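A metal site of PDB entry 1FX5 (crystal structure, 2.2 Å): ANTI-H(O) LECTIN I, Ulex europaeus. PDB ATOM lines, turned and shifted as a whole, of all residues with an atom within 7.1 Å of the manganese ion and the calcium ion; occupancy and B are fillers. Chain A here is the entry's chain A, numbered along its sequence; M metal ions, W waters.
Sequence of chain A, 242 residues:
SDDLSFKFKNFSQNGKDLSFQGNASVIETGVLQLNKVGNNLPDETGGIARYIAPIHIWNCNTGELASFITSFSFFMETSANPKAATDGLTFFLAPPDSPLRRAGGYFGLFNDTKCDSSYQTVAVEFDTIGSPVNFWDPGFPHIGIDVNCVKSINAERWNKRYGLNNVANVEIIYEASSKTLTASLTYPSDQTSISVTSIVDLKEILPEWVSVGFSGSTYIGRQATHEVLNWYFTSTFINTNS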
ATOM      1  N   ASP A  87      13.328 -16.578 -30.528  1.00  0.00           N
ATOM      2  CA  ASP A  87      13.923 -15.310 -30.065  1.00  0.00           C
ATOM      3  C   ASP A  87      13.646 -14.177 -31.044  1.00  0.00           C
ATOM      4  O   ASP A  87      13.801 -13.007 -30.676  1.00  0.00           O
ATOM      5  CB  ASP A  87      15.431 -15.425 -29.872  1.00  0.00           C
ATOM      6  CG  ASP A  87      15.801 -15.866 -28.497  1.00  0.00           C
ATOM      7  OD1 ASP A  87      16.064 -17.076 -28.330  1.00  0.00           O
ATOM      8  OD2 ASP A  87      15.786 -15.033 -27.571  1.00  0.00           O
ATOM      9  N   GLY A 104      20.393 -17.866 -29.932  1.00  0.00           N
ATOM     10  CA  GLY A 104      19.561 -17.554 -28.785  1.00  0.00           C
ATOM     11  C   GLY A 104      19.230 -16.066 -28.845  1.00  0.00           C
ATOM     12  O   GLY A 104      19.062 -15.530 -29.937  1.00  0.00           O
ATOM     13  N   GLY A 105      19.217 -15.362 -27.703  1.00  0.00           N
ATOM     14  CA  GLY A 105      18.896 -13.944 -27.730  1.00  0.00           C
ATOM     15  C   GLY A 105      19.923 -13.004 -28.363  1.00  0.00           C
ATOM     16  O   GLY A 105      19.741 -11.787 -28.383  1.00  0.00           O
ATOM     17  N   TYR A 106      21.003 -13.554 -28.885  1.00  0.00           N
ATOM     18  CA  TYR A 106      22.042 -12.757 -29.509  1.00  0.00           C
ATOM     19  C   TYR A 106      21.937 -12.803 -31.042  1.00  0.00           C
ATOM     20  O   TYR A 106      22.814 -12.267 -31.751  1.00  0.00           O
ATOM     21  CB  TYR A 106      23.417 -13.156 -28.972  1.00  0.00           C
ATOM     22  CG  TYR A 106      23.561 -12.897 -27.485  1.00  0.00           C
ATOM     23  CD1 TYR A 106      23.510 -13.939 -26.571  1.00  0.00           C
ATOM     24  CD2 TYR A 106      23.737 -11.619 -27.000  1.00  0.00           C
ATOM     25  CE1 TYR A 106      23.642 -13.701 -25.202  1.00  0.00           C
ATOM     26  CE2 TYR A 106      23.867 -11.365 -25.629  1.00  0.00           C
ATOM     27  CZ  TYR A 106      23.816 -12.413 -24.745  1.00  0.00           C
ATOM     28  OH  TYR A 106      23.991 -12.176 -23.397  1.00  0.00           O
ATOM     29  N   PHE A 107      20.907 -13.495 -31.552  1.00  0.00           N
ATOM     30  CA  PHE A 107      20.609 -13.651 -32.984  1.00  0.00           C
ATOM     31  C   PHE A 107      21.678 -14.116 -33.956  1.00  0.00           C
ATOM     32  O   PHE A 107      21.503 -13.945 -35.187  1.00  0.00           O
ATOM     33  CB  PHE A 107      20.081 -12.312 -33.552  1.00  0.00           C
ATOM     34  CG  PHE A 107      18.909 -11.753 -32.812  1.00  0.00           C
ATOM     35  CD1 PHE A 107      19.046 -10.628 -31.989  1.00  0.00           C
ATOM     36  CD2 PHE A 107      17.655 -12.332 -32.930  1.00  0.00           C
ATOM     37  CE1 PHE A 107      17.964 -10.102 -31.297  1.00  0.00           C
ATOM     38  CE2 PHE A 107      16.564 -11.810 -32.228  1.00  0.00           C
ATOM     39  CZ  PHE A 107      16.727 -10.696 -31.414  1.00  0.00           C
ATOM     40  N   GLU A 125      15.871  -5.468 -35.788  1.00  0.00           N
ATOM     41  CA  GLU A 125      15.394  -6.669 -35.108  1.00  0.00           C
ATOM     42  C   GLU A 125      13.875  -6.719 -34.801  1.00  0.00           C
ATOM     43  O   GLU A 125      13.247  -5.712 -34.473  1.00  0.00           O
ATOM     44  CB  GLU A 125      16.187  -6.915 -33.799  1.00  0.00           C
ATOM     45  CG  GLU A 125      15.962  -5.824 -32.745  1.00  0.00           C
ATOM     46  CD  GLU A 125      16.561  -6.133 -31.389  1.00  0.00           C
ATOM     47  OE1 GLU A 125      15.894  -5.880 -30.369  1.00  0.00           O
ATOM     48  OE2 GLU A 125      17.702  -6.614 -31.310  1.00  0.00           O
ATOM     49  N   PHE A 126      13.330  -7.934 -34.908  1.00  0.00           N
ATOM     50  CA  PHE A 126      11.932  -8.302 -34.663  1.00  0.00           C
ATOM     51  C   PHE A 126      12.171  -9.279 -33.504  1.00  0.00           C
ATOM     52  O   PHE A 126      12.276 -10.514 -33.693  1.00  0.00           O
ATOM     53  CB  PHE A 126      11.350  -8.982 -35.911  1.00  0.00           C
ATOM     54  CG  PHE A 126      11.354  -8.083 -37.142  1.00  0.00           C
ATOM     55  CD1 PHE A 126      12.405  -8.147 -38.045  1.00  0.00           C
ATOM     56  CD2 PHE A 126      10.345  -7.136 -37.349  1.00  0.00           C
ATOM     57  CE1 PHE A 126      12.446  -7.269 -39.118  1.00  0.00           C
ATOM     58  CE2 PHE A 126      10.392  -6.266 -38.440  1.00  0.00           C
ATOM     59  CZ  PHE A 126      11.444  -6.327 -39.320  1.00  0.00           C
ATOM     60  N   ASP A 127      12.358  -8.678 -32.334  1.00  0.00           N
ATOM     61  CA  ASP A 127      12.632  -9.349 -31.082  1.00  0.00           C
ATOM     62  C   ASP A 127      11.391  -9.845 -30.358  1.00  0.00           C
ATOM     63  O   ASP A 127      10.630  -9.044 -29.788  1.00  0.00           O
ATOM     64  CB  ASP A 127      13.446  -8.359 -30.237  1.00  0.00           C
ATOM     65  CG  ASP A 127      14.151  -9.020 -29.070  1.00  0.00           C
ATOM     66  OD1 ASP A 127      15.126  -8.438 -28.541  1.00  0.00           O
ATOM     67  OD2 ASP A 127      13.738 -10.107 -28.658  1.00  0.00           O
ATOM     68  N   THR A 128      11.254 -11.175 -30.287  1.00  0.00           N
ATOM     69  CA  THR A 128      10.097 -11.781 -29.625  1.00  0.00           C
ATOM     70  C   THR A 128      10.112 -11.953 -28.104  1.00  0.00           C
ATOM     71  O   THR A 128       9.114 -12.420 -27.543  1.00  0.00           O
ATOM     72  CB  THR A 128       9.683 -13.110 -30.310  1.00  0.00           C
ATOM     73  OG1 THR A 128      10.745 -14.061 -30.165  1.00  0.00           O
ATOM     74  CG2 THR A 128       9.403 -12.901 -31.794  1.00  0.00           C
ATOM     75  N   ILE A 129      11.222 -11.627 -27.433  1.00  0.00           N
ATOM     76  CA  ILE A 129      11.293 -11.749 -25.961  1.00  0.00           C
ATOM     77  C   ILE A 129      12.199 -10.674 -25.329  1.00  0.00           C
ATOM     78  O   ILE A 129      13.347 -10.480 -25.769  1.00  0.00           O
ATOM     79  CB  ILE A 129      11.740 -13.184 -25.514  1.00  0.00           C
ATOM     80  CG1 ILE A 129      11.347 -13.435 -24.051  1.00  0.00           C
ATOM     81  CG2 ILE A 129      13.248 -13.401 -25.707  1.00  0.00           C
ATOM     82  CD1 ILE A 129       9.877 -13.894 -23.847  1.00  0.00           C
ATOM     83  N   GLY A 130      11.666  -9.975 -24.313  1.00  0.00           N
ATOM     84  CA  GLY A 130      12.417  -8.926 -23.605  1.00  0.00           C
ATOM     85  C   GLY A 130      12.789  -9.220 -22.146  1.00  0.00           C
ATOM     86  O   GLY A 130      12.958 -10.383 -21.779  1.00  0.00           O
ATOM     87  N   SER A 131      12.951  -8.195 -21.305  1.00  0.00           N
ATOM     88  CA  SER A 131      13.296  -8.448 -19.906  1.00  0.00           C
ATOM     89  C   SER A 131      12.068  -9.011 -19.194  1.00  0.00           C
ATOM     90  O   SER A 131      10.935  -8.691 -19.564  1.00  0.00           O
ATOM     91  CB  SER A 131      13.780  -7.179 -19.206  1.00  0.00           C
ATOM     92  OG  SER A 131      12.844  -6.141 -19.373  1.00  0.00           O
ATOM     93  N   VAL A 133      13.760 -11.991 -19.045  1.00  0.00           N
ATOM     94  CA  VAL A 133      14.505 -13.030 -19.766  1.00  0.00           C
ATOM     95  C   VAL A 133      15.774 -12.493 -20.420  1.00  0.00           C
ATOM     96  O   VAL A 133      16.801 -13.152 -20.401  1.00  0.00           O
ATOM     97  CB  VAL A 133      13.614 -13.751 -20.786  1.00  0.00           C
ATOM     98  CG1 VAL A 133      14.401 -14.839 -21.496  1.00  0.00           C
ATOM     99  CG2 VAL A 133      12.407 -14.359 -20.071  1.00  0.00           C
ATOM    100  N   ASN A 134      15.670 -11.323 -21.053  1.00  0.00           N
ATOM    101  CA  ASN A 134      16.811 -10.687 -21.699  1.00  0.00           C
ATOM    102  C   ASN A 134      16.882  -9.366 -20.936  1.00  0.00           C
ATOM    103  O   ASN A 134      16.109  -8.450 -21.214  1.00  0.00           O
ATOM    104  CB  ASN A 134      16.528 -10.420 -23.175  1.00  0.00           C
ATOM    105  CG  ASN A 134      16.640 -11.676 -24.034  1.00  0.00           C
ATOM    106  OD1 ASN A 134      16.318 -11.677 -25.224  1.00  0.00           O
ATOM    107  ND2 ASN A 134      17.099 -12.760 -23.429  1.00  0.00           N
ATOM    108  N   TRP A 136      18.779  -6.818 -21.078  1.00  0.00           N
ATOM    109  CA  TRP A 136      19.124  -5.606 -21.827  1.00  0.00           C
ATOM    110  C   TRP A 136      18.003  -4.998 -22.682  1.00  0.00           C
ATOM    111  O   TRP A 136      18.202  -3.958 -23.300  1.00  0.00           O
ATOM    112  CB  TRP A 136      20.295  -5.927 -22.762  1.00  0.00           C
ATOM    113  CG  TRP A 136      20.036  -7.139 -23.631  1.00  0.00           C
ATOM    114  CD1 TRP A 136      19.452  -7.149 -24.888  1.00  0.00           C
ATOM    115  CD2 TRP A 136      20.350  -8.504 -23.312  1.00  0.00           C
ATOM    116  NE1 TRP A 136      19.391  -8.445 -25.353  1.00  0.00           N
ATOM    117  CE2 TRP A 136      19.945  -9.291 -24.413  1.00  0.00           C
ATOM    118  CE3 TRP A 136      20.934  -9.136 -22.207  1.00  0.00           C
ATOM    119  CZ2 TRP A 136      20.112 -10.675 -24.438  1.00  0.00           C
ATOM    120  CZ3 TRP A 136      21.101 -10.520 -22.232  1.00  0.00           C
ATOM    121  CH2 TRP A 136      20.691 -11.264 -23.342  1.00  0.00           C
ATOM    122  N   ASP A 137      16.860  -5.701 -22.790  1.00  0.00           N
ATOM    123  CA  ASP A 137      15.689  -5.278 -23.568  1.00  0.00           C
ATOM    124  C   ASP A 137      14.572  -4.573 -22.784  1.00  0.00           C
ATOM    125  O   ASP A 137      14.577  -4.594 -21.548  1.00  0.00           O
ATOM    126  CB  ASP A 137      14.985  -6.522 -24.143  1.00  0.00           C
ATOM    127  CG  ASP A 137      15.679  -7.122 -25.333  1.00  0.00           C
ATOM    128  OD1 ASP A 137      15.599  -8.384 -25.444  1.00  0.00           O
ATOM    129  OD2 ASP A 137      16.253  -6.378 -26.158  1.00  0.00           O
ATOM    130  N   PRO A 138      13.605  -3.916 -23.487  1.00  0.00           N
ATOM    131  CA  PRO A 138      12.501  -3.286 -22.769  1.00  0.00           C
ATOM    132  C   PRO A 138      11.653  -4.500 -22.278  1.00  0.00           C
ATOM    133  O   PRO A 138      11.837  -5.625 -22.763  1.00  0.00           O
ATOM    134  CB  PRO A 138      11.776  -2.475 -23.860  1.00  0.00           C
ATOM    135  CG  PRO A 138      12.314  -3.011 -25.171  1.00  0.00           C
ATOM    136  CD  PRO A 138      13.718  -3.377 -24.856  1.00  0.00           C
ATOM    137  N   PHE A 140       8.998  -6.169 -22.984  1.00  0.00           N
ATOM    138  CA  PHE A 140       7.970  -6.698 -23.892  1.00  0.00           C
ATOM    139  C   PHE A 140       8.550  -6.923 -25.292  1.00  0.00           C
ATOM    140  O   PHE A 140       9.647  -6.445 -25.577  1.00  0.00           O
ATOM    141  CB  PHE A 140       6.793  -5.709 -24.011  1.00  0.00           C
ATOM    142  CG  PHE A 140       7.190  -4.244 -23.992  1.00  0.00           C
ATOM    143  CD1 PHE A 140       6.914  -3.448 -22.882  1.00  0.00           C
ATOM    144  CD2 PHE A 140       7.854  -3.674 -25.076  1.00  0.00           C
ATOM    145  CE1 PHE A 140       7.299  -2.119 -22.853  1.00  0.00           C
ATOM    146  CE2 PHE A 140       8.246  -2.338 -25.048  1.00  0.00           C
ATOM    147  CZ  PHE A 140       7.964  -1.561 -23.931  1.00  0.00           C
ATOM    148  N   HIS A 142       9.401  -6.443 -29.173  1.00  0.00           N
ATOM    149  CA  HIS A 142       9.580  -5.133 -29.813  1.00  0.00           C
ATOM    150  C   HIS A 142      10.391  -5.167 -31.099  1.00  0.00           C
ATOM    151  O   HIS A 142      11.024  -6.189 -31.408  1.00  0.00           O
ATOM    152  CB  HIS A 142      10.365  -4.268 -28.809  1.00  0.00           C
ATOM    153  CG  HIS A 142      11.645  -4.927 -28.325  1.00  0.00           C
ATOM    154  ND1 HIS A 142      11.681  -5.965 -27.408  1.00  0.00           N
ATOM    155  CD2 HIS A 142      12.931  -4.723 -28.703  1.00  0.00           C
ATOM    156  CE1 HIS A 142      12.956  -6.365 -27.265  1.00  0.00           C
ATOM    157  NE2 HIS A 142      13.765  -5.642 -28.019  1.00  0.00           N
ATOM    158  N   ILE A 143      10.278  -4.114 -31.923  1.00  0.00           N
ATOM    159  CA  ILE A 143      11.072  -4.084 -33.151  1.00  0.00           C
ATOM    160  C   ILE A 143      12.080  -2.941 -32.879  1.00  0.00           C
ATOM    161  O   ILE A 143      11.691  -1.853 -32.408  1.00  0.00           O
ATOM    162  CB  ILE A 143      10.292  -3.913 -34.525  1.00  0.00           C
ATOM    163  CG1 ILE A 143      10.074  -2.454 -34.900  1.00  0.00           C
ATOM    164  CG2 ILE A 143       9.008  -4.701 -34.516  1.00  0.00           C
ATOM    165  CD1 ILE A 143       9.034  -1.742 -34.073  1.00  0.00           C
ATOM    166  N   GLY A 144      13.379  -3.226 -33.052  1.00  0.00           N
ATOM    167  CA  GLY A 144      14.372  -2.196 -32.804  1.00  0.00           C
ATOM    168  C   GLY A 144      15.524  -2.064 -33.783  1.00  0.00           C
ATOM    169  O   GLY A 144      15.717  -2.890 -34.690  1.00  0.00           O
ATOM    170  N   ASP A 146      19.559  -1.823 -34.077  1.00  0.00           N
ATOM    171  CA  ASP A 146      20.829  -2.123 -33.412  1.00  0.00           C
ATOM    172  C   ASP A 146      22.029  -1.626 -34.183  1.00  0.00           C
ATOM    173  O   ASP A 146      22.160  -1.891 -35.377  1.00  0.00           O
ATOM    174  CB  ASP A 146      21.007  -3.632 -33.232  1.00  0.00           C
ATOM    175  CG  ASP A 146      19.866  -4.293 -32.484  1.00  0.00           C
ATOM    176  OD1 ASP A 146      19.029  -3.605 -31.866  1.00  0.00           O
ATOM    177  OD2 ASP A 146      19.802  -5.514 -32.505  1.00  0.00           O
ATOM    178  N   VAL A 150      23.844  -5.587 -29.119  1.00  0.00           N
ATOM    179  CA  VAL A 150      22.567  -6.294 -28.984  1.00  0.00           C
ATOM    180  C   VAL A 150      21.529  -5.352 -28.301  1.00  0.00           C
ATOM    181  O   VAL A 150      20.332  -5.626 -28.295  1.00  0.00           O
ATOM    182  CB  VAL A 150      22.722  -7.660 -28.203  1.00  0.00           C
ATOM    183  CG1 VAL A 150      23.000  -7.424 -26.710  1.00  0.00           C
ATOM    184  CG2 VAL A 150      21.474  -8.540 -28.404  1.00  0.00           C
ATOM    185  N   LYS A 151      22.025  -4.271 -27.709  1.00  0.00           N
ATOM    186  CA  LYS A 151      21.149  -3.301 -27.044  1.00  0.00           C
ATOM    187  C   LYS A 151      20.786  -2.240 -28.108  1.00  0.00           C
ATOM    188  O   LYS A 151      21.688  -1.700 -28.742  1.00  0.00           O
ATOM    189  CB  LYS A 151      21.889  -2.639 -25.886  1.00  0.00           C
ATOM    190  CG  LYS A 151      21.024  -1.707 -25.065  1.00  0.00           C
ATOM    191  CD  LYS A 151      21.835  -1.162 -23.914  1.00  0.00           C
ATOM    192  CE  LYS A 151      20.963  -0.411 -22.926  1.00  0.00           C
ATOM    193  NZ  LYS A 151      19.964  -1.291 -22.265  1.00  0.00           N
ATOM    194  N   SER A 152      19.499  -1.989 -28.326  1.00  0.00           N
ATOM    195  CA  SER A 152      19.044  -1.011 -29.326  1.00  0.00           C
ATOM    196  C   SER A 152      19.167   0.481 -28.962  1.00  0.00           C
ATOM    197  O   SER A 152      19.150   0.835 -27.771  1.00  0.00           O
ATOM    198  CB  SER A 152      17.558  -1.255 -29.628  1.00  0.00           C
ATOM    199  OG  SER A 152      17.256  -2.618 -29.912  1.00  0.00           O
ATOM    200  N   ALA A 155      13.646   1.581 -29.968  1.00  0.00           N
ATOM    201  CA  ALA A 155      12.792   0.393 -30.092  1.00  0.00           C
ATOM    202  C   ALA A 155      11.311   0.750 -29.883  1.00  0.00           C
ATOM    203  O   ALA A 155      11.018   1.735 -29.201  1.00  0.00           O
ATOM    204  CB  ALA A 155      13.208  -0.649 -29.042  1.00  0.00           C
HETATM  205 MN    MN M   1      15.965  -6.463 -28.266  1.00  0.00          MN
HETATM  206 CA    CA M   2      15.447 -10.355 -26.857  1.00  0.00          CA
HETATM  207  O   HOH W   1      15.338 -12.273 -28.120  1.00  0.00           O
HETATM  208  O   HOH W   2      16.536  -4.359 -27.994  1.00  0.00           O
HETATM  209  O   HOH W   3      17.604  -9.940 -27.667  1.00  0.00           O
HETATM  210  O   HOH W   4      17.965  -7.060 -28.639  1.00  0.00           O
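The backbone carbonyl oxygen (O) of Phe 140 sits at hydrogen-bond distance from a ring nitrogen (ND1) of His 142 (2.8 Å). OE2 of Glu 125 lies close to OD2 of Asp 146 (2.7 Å). The backbone carbonyl oxygen (O) of Gly 144 lies within hydrogen-bond range of the backbone NH (N) of Glu 125 (2.8 Å). OG of Ser 131 is in hydrogen-bond range of O of Asp 137 (3.2 Å).
Four residues have an atom within 4 Å of the manganese ion: Glu 125, Asp 127, Asp 137 and His 142. Along chain A the residues within 4 Å of the manganese ion span positions 125 to 142.
Of the 26 residues printed, 4 come within 4 Å of the calcium ion. The nearest printed residue that does not touch the calcium ion is Gly 130 (4.6 Å).
The manganese ion is bound by water W4, OD2 of Asp 137, OD1 of Asp 127, OE1 of Glu 125, water W2 and NE2 of His 142.
The calcium ion is bound by the side-chain amide oxygen (OD1) of Asn 134 (2.3 Å), water W1 (2.3 Å), water W3 (2.3 Å), the backbone carbonyl oxygen (O) of Ile 129 (2.4 Å), the side-chain carboxylate (OD1) of Asp 137 (2.4 Å), the side-chain carboxylate (OD2) of Asp 127 (2.5 Å) and the side-chain carboxylate (OD1) of Asp 127 (2.6 Å).
Water W4 lies within hydrogen-bond range of the side-chain carboxylate of Glu 125 (2.7 Å) and the backbone carbonyl oxygen of Val 150 (2.8 Å). Water W3 bridges the backbone carbonyl oxygen of Gly 105 (2.9 Å) and the indole nitrogen of Trp 136 (3.3 Å).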
